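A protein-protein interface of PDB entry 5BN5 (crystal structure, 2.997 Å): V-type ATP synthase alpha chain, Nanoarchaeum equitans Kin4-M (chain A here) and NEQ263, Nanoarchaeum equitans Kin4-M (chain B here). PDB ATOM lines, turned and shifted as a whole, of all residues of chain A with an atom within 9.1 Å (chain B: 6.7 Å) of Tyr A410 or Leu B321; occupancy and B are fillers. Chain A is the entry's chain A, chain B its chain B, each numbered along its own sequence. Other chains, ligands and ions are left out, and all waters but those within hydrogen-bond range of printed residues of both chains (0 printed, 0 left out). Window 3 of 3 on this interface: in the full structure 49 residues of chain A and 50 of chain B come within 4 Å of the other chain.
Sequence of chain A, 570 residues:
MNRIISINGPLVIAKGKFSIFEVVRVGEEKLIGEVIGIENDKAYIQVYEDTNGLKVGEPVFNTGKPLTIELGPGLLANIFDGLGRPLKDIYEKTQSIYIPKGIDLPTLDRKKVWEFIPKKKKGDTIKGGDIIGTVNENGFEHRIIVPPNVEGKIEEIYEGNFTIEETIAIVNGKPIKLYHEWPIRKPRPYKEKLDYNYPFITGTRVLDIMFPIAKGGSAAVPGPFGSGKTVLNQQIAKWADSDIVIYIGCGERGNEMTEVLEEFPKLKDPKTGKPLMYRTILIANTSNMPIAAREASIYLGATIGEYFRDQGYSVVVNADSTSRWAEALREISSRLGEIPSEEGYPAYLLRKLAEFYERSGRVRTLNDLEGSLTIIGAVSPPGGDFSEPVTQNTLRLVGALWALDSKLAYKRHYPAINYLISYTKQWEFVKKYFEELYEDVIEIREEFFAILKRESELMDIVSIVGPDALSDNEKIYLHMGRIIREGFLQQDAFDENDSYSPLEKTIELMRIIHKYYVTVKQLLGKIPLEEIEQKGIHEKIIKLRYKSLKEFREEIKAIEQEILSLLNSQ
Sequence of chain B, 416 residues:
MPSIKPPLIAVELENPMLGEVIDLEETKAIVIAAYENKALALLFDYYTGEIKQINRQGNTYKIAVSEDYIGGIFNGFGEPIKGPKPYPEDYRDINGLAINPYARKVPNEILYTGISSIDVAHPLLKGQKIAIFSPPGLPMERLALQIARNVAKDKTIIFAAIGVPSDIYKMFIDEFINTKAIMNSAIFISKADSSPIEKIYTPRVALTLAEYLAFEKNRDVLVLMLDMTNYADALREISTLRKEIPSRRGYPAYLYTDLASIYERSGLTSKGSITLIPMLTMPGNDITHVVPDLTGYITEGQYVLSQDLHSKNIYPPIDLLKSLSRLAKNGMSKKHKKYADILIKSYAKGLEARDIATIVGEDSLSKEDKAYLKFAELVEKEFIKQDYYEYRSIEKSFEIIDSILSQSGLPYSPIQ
The backbone carbonyl oxygen (O) of Leu B321 sits at hydrogen-bond distance from the guanidinium group (NH1) of Arg A412. NH2 of Arg A412 lies within hydrogen-bond range of O of Ser B323, at 3.0 Å.
OD1 of Asp B319 sits at hydrogen-bond distance from N of Leu B321, at 3.0 Å. OH of Tyr A414 is in hydrogen-bond range of O of Gly A226, 3.4 Å away. The side-chain carboxylate of Asp B319 lies within hydrogen-bond range of the backbone NH of Lys B322 (2.6 Å). O of Asp B319 lies within hydrogen-bond range of OG of Ser B323. O of Leu B320 sits at hydrogen-bond distance from NE2 of His B122 (2.8 Å).
Among the printed residues, pairs that only touch across the chains: Gly A226 with Leu B324 (3.6 Å), Tyr A410 with Leu B321 (3.5 Å), Tyr A410 with Lys B322 (3.9 Å), Arg A412 with His B122 (3.2 Å), Arg A412 with Leu B324 (3.9 Å) and Arg A412 with Ile B344 (3.97 Å).
Leu A404 touches none of the printed residues of chain B. Tyr A410 touches just these residues of chain B: Leu B321 and Lys B322. Printed residues of chain B within 4 Å of Arg A412: His B122, Leu B321, Ser B323, Leu B324 and Ile B344. Of the printed residues of chain A, His B122 touches Arg A412. Of chain A, only Tyr A410 (3.5 Å) and Arg A412 (2.7 Å) come within 4 Å of Leu B321. Leu B343 touches none of the printed residues of chain A.
Of the 15 printed residues of chain B, 6 touch a printed residue of chain A. Hydrophobic or aromatic side chains of chain A within 4 Å of the printed part of chain B: Tyr A410. Among the printed residues, no Asp or Glu carboxylate lies within 4 Å of a Lys or Arg side-chain nitrogen of the other chain.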
ATOM      1  N   PRO A 224     -17.122  17.171   2.769  1.00  0.00           N
ATOM      2  CA  PRO A 224     -18.208  18.155   2.809  1.00  0.00           C
ATOM      3  C   PRO A 224     -19.578  17.484   2.774  1.00  0.00           C
ATOM      4  O   PRO A 224     -19.662  16.256   2.783  1.00  0.00           O
ATOM      5  CB  PRO A 224     -17.987  18.958   1.526  1.00  0.00           C
ATOM      6  CG  PRO A 224     -17.341  17.992   0.598  1.00  0.00           C
ATOM      7  CD  PRO A 224     -16.454  17.136   1.457  1.00  0.00           C
ATOM      8  N   PHE A 225     -20.637  18.286   2.737  1.00  0.00           N
ATOM      9  CA  PHE A 225     -21.993  17.752   2.675  1.00  0.00           C
ATOM     10  C   PHE A 225     -22.324  17.262   1.270  1.00  0.00           C
ATOM     11  O   PHE A 225     -21.786  17.767   0.284  1.00  0.00           O
ATOM     12  CB  PHE A 225     -23.015  18.795   3.136  1.00  0.00           C
ATOM     13  CG  PHE A 225     -22.967  20.084   2.364  1.00  0.00           C
ATOM     14  CD1 PHE A 225     -22.123  21.111   2.754  1.00  0.00           C
ATOM     15  CD2 PHE A 225     -23.774  20.273   1.253  1.00  0.00           C
ATOM     16  CE1 PHE A 225     -22.078  22.297   2.049  1.00  0.00           C
ATOM     17  CE2 PHE A 225     -23.734  21.459   0.544  1.00  0.00           C
ATOM     18  CZ  PHE A 225     -22.885  22.472   0.941  1.00  0.00           C
ATOM     19  N   GLY A 226     -23.210  16.275   1.186  1.00  0.00           N
ATOM     20  CA  GLY A 226     -23.587  15.696  -0.089  1.00  0.00           C
ATOM     21  C   GLY A 226     -22.618  14.614  -0.522  1.00  0.00           C
ATOM     22  O   GLY A 226     -22.777  14.009  -1.582  1.00  0.00           O
ATOM     23  N   SER A 227     -21.607  14.374   0.306  1.00  0.00           N
ATOM     24  CA  SER A 227     -20.594  13.368   0.015  1.00  0.00           C
ATOM     25  C   SER A 227     -21.125  11.964   0.277  1.00  0.00           C
ATOM     26  O   SER A 227     -21.074  11.098  -0.595  1.00  0.00           O
ATOM     27  CB  SER A 227     -19.338  13.625   0.850  1.00  0.00           C
ATOM     28  OG  SER A 227     -19.636  13.613   2.236  1.00  0.00           O
ATOM     29  N   LEU A 404     -13.850  11.621   1.431  1.00  0.00           N
ATOM     30  CA  LEU A 404     -14.889  11.731   0.414  1.00  0.00           C
ATOM     31  C   LEU A 404     -14.666  12.971  -0.446  1.00  0.00           C
ATOM     32  O   LEU A 404     -14.684  14.096   0.053  1.00  0.00           O
ATOM     33  CB  LEU A 404     -16.272  11.770   1.063  1.00  0.00           C
ATOM     34  CG  LEU A 404     -16.746  10.458   1.693  1.00  0.00           C
ATOM     35  CD1 LEU A 404     -18.004  10.672   2.518  1.00  0.00           C
ATOM     36  CD2 LEU A 404     -16.984   9.413   0.616  1.00  0.00           C
ATOM     37  N   ASP A 405     -14.456  12.755  -1.740  1.00  0.00           N
ATOM     38  CA  ASP A 405     -14.130  13.841  -2.657  1.00  0.00           C
ATOM     39  C   ASP A 405     -15.381  14.497  -3.235  1.00  0.00           C
ATOM     40  O   ASP A 405     -16.397  13.837  -3.455  1.00  0.00           O
ATOM     41  CB  ASP A 405     -13.229  13.330  -3.784  1.00  0.00           C
ATOM     42  CG  ASP A 405     -12.532  14.450  -4.526  1.00  0.00           C
ATOM     43  OD1 ASP A 405     -12.312  15.519  -3.918  1.00  0.00           O
ATOM     44  OD2 ASP A 405     -12.198  14.259  -5.714  1.00  0.00           O
ATOM     45  N   SER A 406     -15.297  15.801  -3.478  1.00  0.00           N
ATOM     46  CA  SER A 406     -16.427  16.565  -3.995  1.00  0.00           C
ATOM     47  C   SER A 406     -16.645  16.317  -5.484  1.00  0.00           C
ATOM     48  O   SER A 406     -17.783  16.227  -5.946  1.00  0.00           O
ATOM     49  CB  SER A 406     -16.222  18.060  -3.744  1.00  0.00           C
ATOM     50  OG  SER A 406     -16.073  18.330  -2.362  1.00  0.00           O
ATOM     51  N   LYS A 407     -15.548  16.212  -6.229  1.00  0.00           N
ATOM     52  CA  LYS A 407     -15.611  16.015  -7.675  1.00  0.00           C
ATOM     53  C   LYS A 407     -16.285  14.696  -8.037  1.00  0.00           C
ATOM     54  O   LYS A 407     -17.014  14.612  -9.025  1.00  0.00           O
ATOM     55  CB  LYS A 407     -14.214  16.087  -8.300  1.00  0.00           C
ATOM     56  CG  LYS A 407     -13.686  17.501  -8.527  1.00  0.00           C
ATOM     57  CD  LYS A 407     -13.236  18.160  -7.230  1.00  0.00           C
ATOM     58  CE  LYS A 407     -12.094  17.390  -6.590  1.00  0.00           C
ATOM     59  NZ  LYS A 407     -11.693  17.972  -5.279  1.00  0.00           N
ATOM     60  N   LEU A 408     -16.036  13.668  -7.232  1.00  0.00           N
ATOM     61  CA  LEU A 408     -16.675  12.373  -7.436  1.00  0.00           C
ATOM     62  C   LEU A 408     -18.147  12.438  -7.045  1.00  0.00           C
ATOM     63  O   LEU A 408     -19.001  11.849  -7.704  1.00  0.00           O
ATOM     64  CB  LEU A 408     -15.957  11.286  -6.634  1.00  0.00           C
ATOM     65  CG  LEU A 408     -14.526  10.963  -7.069  1.00  0.00           C
ATOM     66  CD1 LEU A 408     -13.896   9.940  -6.137  1.00  0.00           C
ATOM     67  CD2 LEU A 408     -14.502  10.469  -8.509  1.00  0.00           C
ATOM     68  N   ALA A 409     -18.438  13.167  -5.973  1.00  0.00           N
ATOM     69  CA  ALA A 409     -19.813  13.346  -5.521  1.00  0.00           C
ATOM     70  C   ALA A 409     -20.571  14.285  -6.452  1.00  0.00           C
ATOM     71  O   ALA A 409     -21.801  14.337  -6.435  1.00  0.00           O
ATOM     72  CB  ALA A 409     -19.838  13.873  -4.094  1.00  0.00           C
ATOM     73  N   TYR A 410     -19.825  15.026  -7.267  1.00  0.00           N
ATOM     74  CA  TYR A 410     -20.411  15.970  -8.211  1.00  0.00           C
ATOM     75  C   TYR A 410     -21.033  15.246  -9.402  1.00  0.00           C
ATOM     76  O   TYR A 410     -22.138  15.576  -9.833  1.00  0.00           O
ATOM     77  CB  TYR A 410     -19.352  16.967  -8.689  1.00  0.00           C
ATOM     78  CG  TYR A 410     -19.885  18.052  -9.595  1.00  0.00           C
ATOM     79  CD1 TYR A 410     -20.604  19.123  -9.080  1.00  0.00           C
ATOM     80  CD2 TYR A 410     -19.659  18.013 -10.965  1.00  0.00           C
ATOM     81  CE1 TYR A 410     -21.090  20.120  -9.904  1.00  0.00           C
ATOM     82  CE2 TYR A 410     -20.140  19.006 -11.797  1.00  0.00           C
ATOM     83  CZ  TYR A 410     -20.855  20.056 -11.261  1.00  0.00           C
ATOM     84  OH  TYR A 410     -21.338  21.048 -12.085  1.00  0.00           O
ATOM     85  N   LYS A 411     -20.319  14.258  -9.930  1.00  0.00           N
ATOM     86  CA  LYS A 411     -20.811  13.479 -11.063  1.00  0.00           C
ATOM     87  C   LYS A 411     -21.539  12.223 -10.594  1.00  0.00           C
ATOM     88  O   LYS A 411     -21.704  11.270 -11.358  1.00  0.00           O
ATOM     89  CB  LYS A 411     -19.661  13.103 -12.001  1.00  0.00           C
ATOM     90  CG  LYS A 411     -18.598  12.223 -11.364  1.00  0.00           C
ATOM     91  CD  LYS A 411     -17.550  11.801 -12.382  1.00  0.00           C
ATOM     92  CE  LYS A 411     -16.515  10.878 -11.760  1.00  0.00           C
ATOM     93  NZ  LYS A 411     -15.507  10.417 -12.754  1.00  0.00           N
ATOM     94  N   ARG A 412     -21.971  12.237  -9.335  1.00  0.00           N
ATOM     95  CA  ARG A 412     -22.696  11.120  -8.731  1.00  0.00           C
ATOM     96  C   ARG A 412     -21.921   9.803  -8.775  1.00  0.00           C
ATOM     97  O   ARG A 412     -22.456   8.767  -9.170  1.00  0.00           O
ATOM     98  CB  ARG A 412     -24.085  10.955  -9.361  1.00  0.00           C
ATOM     99  CG  ARG A 412     -25.204  11.654  -8.598  1.00  0.00           C
ATOM    100  CD  ARG A 412     -25.001  13.161  -8.542  1.00  0.00           C
ATOM    101  NE  ARG A 412     -25.972  13.810  -7.665  1.00  0.00           N
ATOM    102  CZ  ARG A 412     -26.043  15.123  -7.469  1.00  0.00           C
ATOM    103  NH1 ARG A 412     -25.200  15.934  -8.092  1.00  0.00           N
ATOM    104  NH2 ARG A 412     -26.960  15.624  -6.652  1.00  0.00           N
ATOM    105  N   HIS A 413     -20.658   9.856  -8.365  1.00  0.00           N
ATOM    106  CA  HIS A 413     -19.824   8.664  -8.266  1.00  0.00           C
ATOM    107  C   HIS A 413     -19.762   8.211  -6.811  1.00  0.00           C
ATOM    108  O   HIS A 413     -18.861   8.602  -6.070  1.00  0.00           O
ATOM    109  CB  HIS A 413     -18.416   8.956  -8.794  1.00  0.00           C
ATOM    110  CG  HIS A 413     -17.464   7.806  -8.665  1.00  0.00           C
ATOM    111  ND1 HIS A 413     -16.846   7.481  -7.477  1.00  0.00           N
ATOM    112  CD2 HIS A 413     -17.012   6.917  -9.580  1.00  0.00           C
ATOM    113  CE1 HIS A 413     -16.063   6.433  -7.663  1.00  0.00           C
ATOM    114  NE2 HIS A 413     -16.146   6.071  -8.930  1.00  0.00           N
ATOM    115  N   TYR A 414     -20.726   7.392  -6.405  1.00  0.00           N
ATOM    116  CA  TYR A 414     -20.808   6.937  -5.020  1.00  0.00           C
ATOM    117  C   TYR A 414     -20.381   5.478  -4.867  1.00  0.00           C
ATOM    118  O   TYR A 414     -20.724   4.639  -5.700  1.00  0.00           O
ATOM    119  CB  TYR A 414     -22.226   7.132  -4.476  1.00  0.00           C
ATOM    120  CG  TYR A 414     -22.677   8.574  -4.453  1.00  0.00           C
ATOM    121  CD1 TYR A 414     -22.299   9.423  -3.421  1.00  0.00           C
ATOM    122  CD2 TYR A 414     -23.482   9.088  -5.461  1.00  0.00           C
ATOM    123  CE1 TYR A 414     -22.709  10.743  -3.395  1.00  0.00           C
ATOM    124  CE2 TYR A 414     -23.897  10.405  -5.444  1.00  0.00           C
ATOM    125  CZ  TYR A 414     -23.507  11.229  -4.408  1.00  0.00           C
ATOM    126  OH  TYR A 414     -23.919  12.541  -4.386  1.00  0.00           O
ATOM    127  N   ALA A 416     -18.005   8.252  -2.956  1.00  0.00           N
ATOM    128  CA  ALA A 416     -17.033   9.208  -3.480  1.00  0.00           C
ATOM    129  C   ALA A 416     -15.691   9.152  -2.756  1.00  0.00           C
ATOM    130  O   ALA A 416     -15.126  10.188  -2.406  1.00  0.00           O
ATOM    131  CB  ALA A 416     -17.604  10.619  -3.432  1.00  0.00           C
ATOM    132  N   HIS B 122     -34.123  15.945  -8.338  1.00  0.00           N
ATOM    133  CA  HIS B 122     -34.118  16.120  -6.887  1.00  0.00           C
ATOM    134  C   HIS B 122     -35.481  16.571  -6.367  1.00  0.00           C
ATOM    135  O   HIS B 122     -35.647  17.727  -5.976  1.00  0.00           O
ATOM    136  CB  HIS B 122     -33.052  17.142  -6.490  1.00  0.00           C
ATOM    137  CG  HIS B 122     -31.807  17.066  -7.319  1.00  0.00           C
ATOM    138  ND1 HIS B 122     -30.811  16.141  -7.086  1.00  0.00           N
ATOM    139  CD2 HIS B 122     -31.397  17.802  -8.379  1.00  0.00           C
ATOM    140  CE1 HIS B 122     -29.842  16.309  -7.968  1.00  0.00           C
ATOM    141  NE2 HIS B 122     -30.173  17.310  -8.765  1.00  0.00           N
ATOM    142  N   ILE B 318     -31.556  26.790 -11.836  1.00  0.00           N
ATOM    143  CA  ILE B 318     -31.122  25.767 -10.893  1.00  0.00           C
ATOM    144  C   ILE B 318     -30.009  24.899 -11.469  1.00  0.00           C
ATOM    145  O   ILE B 318     -30.132  24.363 -12.571  1.00  0.00           O
ATOM    146  CB  ILE B 318     -32.300  24.862 -10.477  1.00  0.00           C
ATOM    147  CG1 ILE B 318     -33.429  25.699  -9.876  1.00  0.00           C
ATOM    148  CG2 ILE B 318     -31.839  23.800  -9.493  1.00  0.00           C
ATOM    149  CD1 ILE B 318     -34.631  24.887  -9.449  1.00  0.00           C
ATOM    150  N   ASP B 319     -28.920  24.768 -10.718  1.00  0.00           N
ATOM    151  CA  ASP B 319     -27.819  23.899 -11.112  1.00  0.00           C
ATOM    152  C   ASP B 319     -28.173  22.451 -10.794  1.00  0.00           C
ATOM    153  O   ASP B 319     -28.277  22.074  -9.628  1.00  0.00           O
ATOM    154  CB  ASP B 319     -26.534  24.298 -10.383  1.00  0.00           C
ATOM    155  CG  ASP B 319     -25.301  23.639 -10.972  1.00  0.00           C
ATOM    156  OD1 ASP B 319     -25.113  22.423 -10.759  1.00  0.00           O
ATOM    157  OD2 ASP B 319     -24.516  24.341 -11.644  1.00  0.00           O
ATOM    158  N   LEU B 320     -28.359  21.646 -11.835  1.00  0.00           N
ATOM    159  CA  LEU B 320     -28.767  20.253 -11.670  1.00  0.00           C
ATOM    160  C   LEU B 320     -27.726  19.412 -10.939  1.00  0.00           C
ATOM    161  O   LEU B 320     -28.069  18.492 -10.199  1.00  0.00           O
ATOM    162  CB  LEU B 320     -29.078  19.622 -13.030  1.00  0.00           C
ATOM    163  CG  LEU B 320     -30.333  20.113 -13.754  1.00  0.00           C
ATOM    164  CD1 LEU B 320     -30.454  19.454 -15.118  1.00  0.00           C
ATOM    165  CD2 LEU B 320     -31.573  19.842 -12.914  1.00  0.00           C
ATOM    166  N   LEU B 321     -26.453  19.732 -11.148  1.00  0.00           N
ATOM    167  CA  LEU B 321     -25.367  18.934 -10.588  1.00  0.00           C
ATOM    168  C   LEU B 321     -24.988  19.359  -9.169  1.00  0.00           C
ATOM    169  O   LEU B 321     -24.473  18.556  -8.394  1.00  0.00           O
ATOM    170  CB  LEU B 321     -24.142  18.981 -11.504  1.00  0.00           C
ATOM    171  CG  LEU B 321     -24.373  18.479 -12.931  1.00  0.00           C
ATOM    172  CD1 LEU B 321     -23.087  18.539 -13.740  1.00  0.00           C
ATOM    173  CD2 LEU B 321     -24.941  17.068 -12.920  1.00  0.00           C
ATOM    174  N   LYS B 322     -25.245  20.620  -8.835  1.00  0.00           N
ATOM    175  CA  LYS B 322     -24.941  21.126  -7.499  1.00  0.00           C
ATOM    176  C   LYS B 322     -26.098  20.902  -6.530  1.00  0.00           C
ATOM    177  O   LYS B 322     -25.886  20.739  -5.329  1.00  0.00           O
ATOM    178  CB  LYS B 322     -24.574  22.610  -7.548  1.00  0.00           C
ATOM    179  CG  LYS B 322     -23.218  22.897  -8.166  1.00  0.00           C
ATOM    180  CD  LYS B 322     -22.900  24.383  -8.119  1.00  0.00           C
ATOM    181  CE  LYS B 322     -21.524  24.675  -8.694  1.00  0.00           C
ATOM    182  NZ  LYS B 322     -21.195  26.126  -8.623  1.00  0.00           N
ATOM    183  N   SER B 323     -27.318  20.899  -7.057  1.00  0.00           N
ATOM    184  CA  SER B 323     -28.505  20.701  -6.231  1.00  0.00           C
ATOM    185  C   SER B 323     -28.538  19.296  -5.640  1.00  0.00           C
ATOM    186  O   SER B 323     -27.931  18.372  -6.180  1.00  0.00           O
ATOM    187  CB  SER B 323     -29.776  20.966  -7.037  1.00  0.00           C
ATOM    188  OG  SER B 323     -29.817  22.311  -7.481  1.00  0.00           O
ATOM    189  N   LEU B 324     -29.253  19.143  -4.531  1.00  0.00           N
ATOM    190  CA  LEU B 324     -29.287  17.871  -3.821  1.00  0.00           C
ATOM    191  C   LEU B 324     -30.628  17.626  -3.134  1.00  0.00           C
ATOM    192  O   LEU B 324     -31.292  18.560  -2.688  1.00  0.00           O
ATOM    193  CB  LEU B 324     -28.153  17.814  -2.791  1.00  0.00           C
ATOM    194  CG  LEU B 324     -28.021  16.550  -1.940  1.00  0.00           C
ATOM    195  CD1 LEU B 324     -27.678  15.348  -2.807  1.00  0.00           C
ATOM    196  CD2 LEU B 324     -26.986  16.742  -0.843  1.00  0.00           C
ATOM    197  N   LEU B 343     -30.596  11.567 -16.807  1.00  0.00           N
ATOM    198  CA  LEU B 343     -30.480  13.019 -16.889  1.00  0.00           C
ATOM    199  C   LEU B 343     -29.143  13.508 -16.342  1.00  0.00           C
ATOM    200  O   LEU B 343     -28.355  14.113 -17.066  1.00  0.00           O
ATOM    201  CB  LEU B 343     -31.626  13.697 -16.136  1.00  0.00           C
ATOM    202  CG  LEU B 343     -31.560  15.223 -16.043  1.00  0.00           C
ATOM    203  CD1 LEU B 343     -31.668  15.856 -17.423  1.00  0.00           C
ATOM    204  CD2 LEU B 343     -32.642  15.753 -15.115  1.00  0.00           C
ATOM    205  N   ILE B 344     -28.895  13.232 -15.065  1.00  0.00           N
ATOM    206  CA  ILE B 344     -27.698  13.716 -14.383  1.00  0.00           C
ATOM    207  C   ILE B 344     -26.394  13.252 -15.035  1.00  0.00           C
ATOM    208  O   ILE B 344     -25.522  14.067 -15.330  1.00  0.00           O
ATOM    209  CB  ILE B 344     -27.701  13.316 -12.891  1.00  0.00           C
ATOM    210  CG1 ILE B 344     -28.827  14.039 -12.150  1.00  0.00           C
ATOM    211  CG2 ILE B 344     -26.361  13.636 -12.246  1.00  0.00           C
ATOM    212  CD1 ILE B 344     -28.710  15.548 -12.186  1.00  0.00           C
ATOM    213  N   LYS B 345     -26.271  11.947 -15.261  1.00  0.00           N
ATOM    214  CA  LYS B 345     -25.047  11.377 -15.822  1.00  0.00           C
ATOM    215  C   LYS B 345     -24.720  11.915 -17.213  1.00  0.00           C
ATOM    216  O   LYS B 345     -23.561  12.191 -17.521  1.00  0.00           O
ATOM    217  CB  LYS B 345     -25.122   9.848 -15.852  1.00  0.00           C
ATOM    218  CG  LYS B 345     -25.072   9.198 -14.480  1.00  0.00           C
ATOM    219  CD  LYS B 345     -25.128   7.683 -14.585  1.00  0.00           C
ATOM    220  CE  LYS B 345     -24.977   7.030 -13.221  1.00  0.00           C
ATOM    221  NZ  LYS B 345     -26.042   7.463 -12.276  1.00  0.00           N
ATOM    222  N   TYR B 347     -25.917  14.768 -18.429  1.00  0.00           N
ATOM    223  CA  TYR B 347     -25.741  16.209 -18.284  1.00  0.00           C
ATOM    224  C   TYR B 347     -24.374  16.521 -17.684  1.00  0.00           C
ATOM    225  O   TYR B 347     -23.767  17.542 -18.002  1.00  0.00           O
ATOM    226  CB  TYR B 347     -26.854  16.802 -17.417  1.00  0.00           C
ATOM    227  CG  TYR B 347     -26.781  18.301 -17.242  1.00  0.00           C
ATOM    228  CD1 TYR B 347     -27.110  19.159 -18.283  1.00  0.00           C
ATOM    229  CD2 TYR B 347     -26.398  18.860 -16.030  1.00  0.00           C
ATOM    230  CE1 TYR B 347     -27.049  20.531 -18.127  1.00  0.00           C
ATOM    231  CE2 TYR B 347     -26.336  20.231 -15.862  1.00  0.00           C
ATOM    232  CZ  TYR B 347     -26.661  21.061 -16.914  1.00  0.00           C
ATOM    233  OH  TYR B 347     -26.600  22.426 -16.752  1.00  0.00           O
ATOM    234  N   ALA B 348     -23.897  15.634 -16.817  1.00  0.00           N
ATOM    235  CA  ALA B 348     -22.578  15.789 -16.215  1.00  0.00           C
ATOM    236  C   ALA B 348     -21.486  15.480 -17.231  1.00  0.00           C
ATOM    237  O   ALA B 348     -20.436  16.122 -17.243  1.00  0.00           O
ATOM    238  CB  ALA B 348     -22.440  14.893 -14.993  1.00  0.00           C
ATOM    239  N   LYS B 349     -21.741  14.493 -18.083  1.00  0.00           N
ATOM    240  CA  LYS B 349     -20.804  14.131 -19.139  1.00  0.00           C
ATOM    241  C   LYS B 349     -20.913  15.130 -20.287  1.00  0.00           C
ATOM    242  O   LYS B 349     -20.007  15.251 -21.110  1.00  0.00           O
ATOM    243  CB  LYS B 349     -21.077  12.709 -19.635  1.00  0.00           C
ATOM    244  CG  LYS B 349     -19.973  12.125 -20.505  1.00  0.00           C
ATOM    245  CD  LYS B 349     -20.273  10.684 -20.886  1.00  0.00           C
ATOM    246  CE  LYS B 349     -19.143  10.083 -21.708  1.00  0.00           C
ATOM    247  NZ  LYS B 349     -17.851  10.093 -20.969  1.00  0.00           N
ATOM    248  N   LEU B 351     -21.554  18.583 -19.776  1.00  0.00           N
ATOM    249  CA  LEU B 351     -20.808  19.757 -19.336  1.00  0.00           C
ATOM    250  C   LEU B 351     -19.314  19.459 -19.339  1.00  0.00           C
ATOM    251  O   LEU B 351     -18.492  20.352 -19.547  1.00  0.00           O
ATOM    252  CB  LEU B 351     -21.252  20.192 -17.938  1.00  0.00           C
ATOM    253  CG  LEU B 351     -22.720  20.588 -17.767  1.00  0.00           C
ATOM    254  CD1 LEU B 351     -22.956  21.164 -16.380  1.00  0.00           C
ATOM    255  CD2 LEU B 351     -23.148  21.572 -18.842  1.00  0.00           C
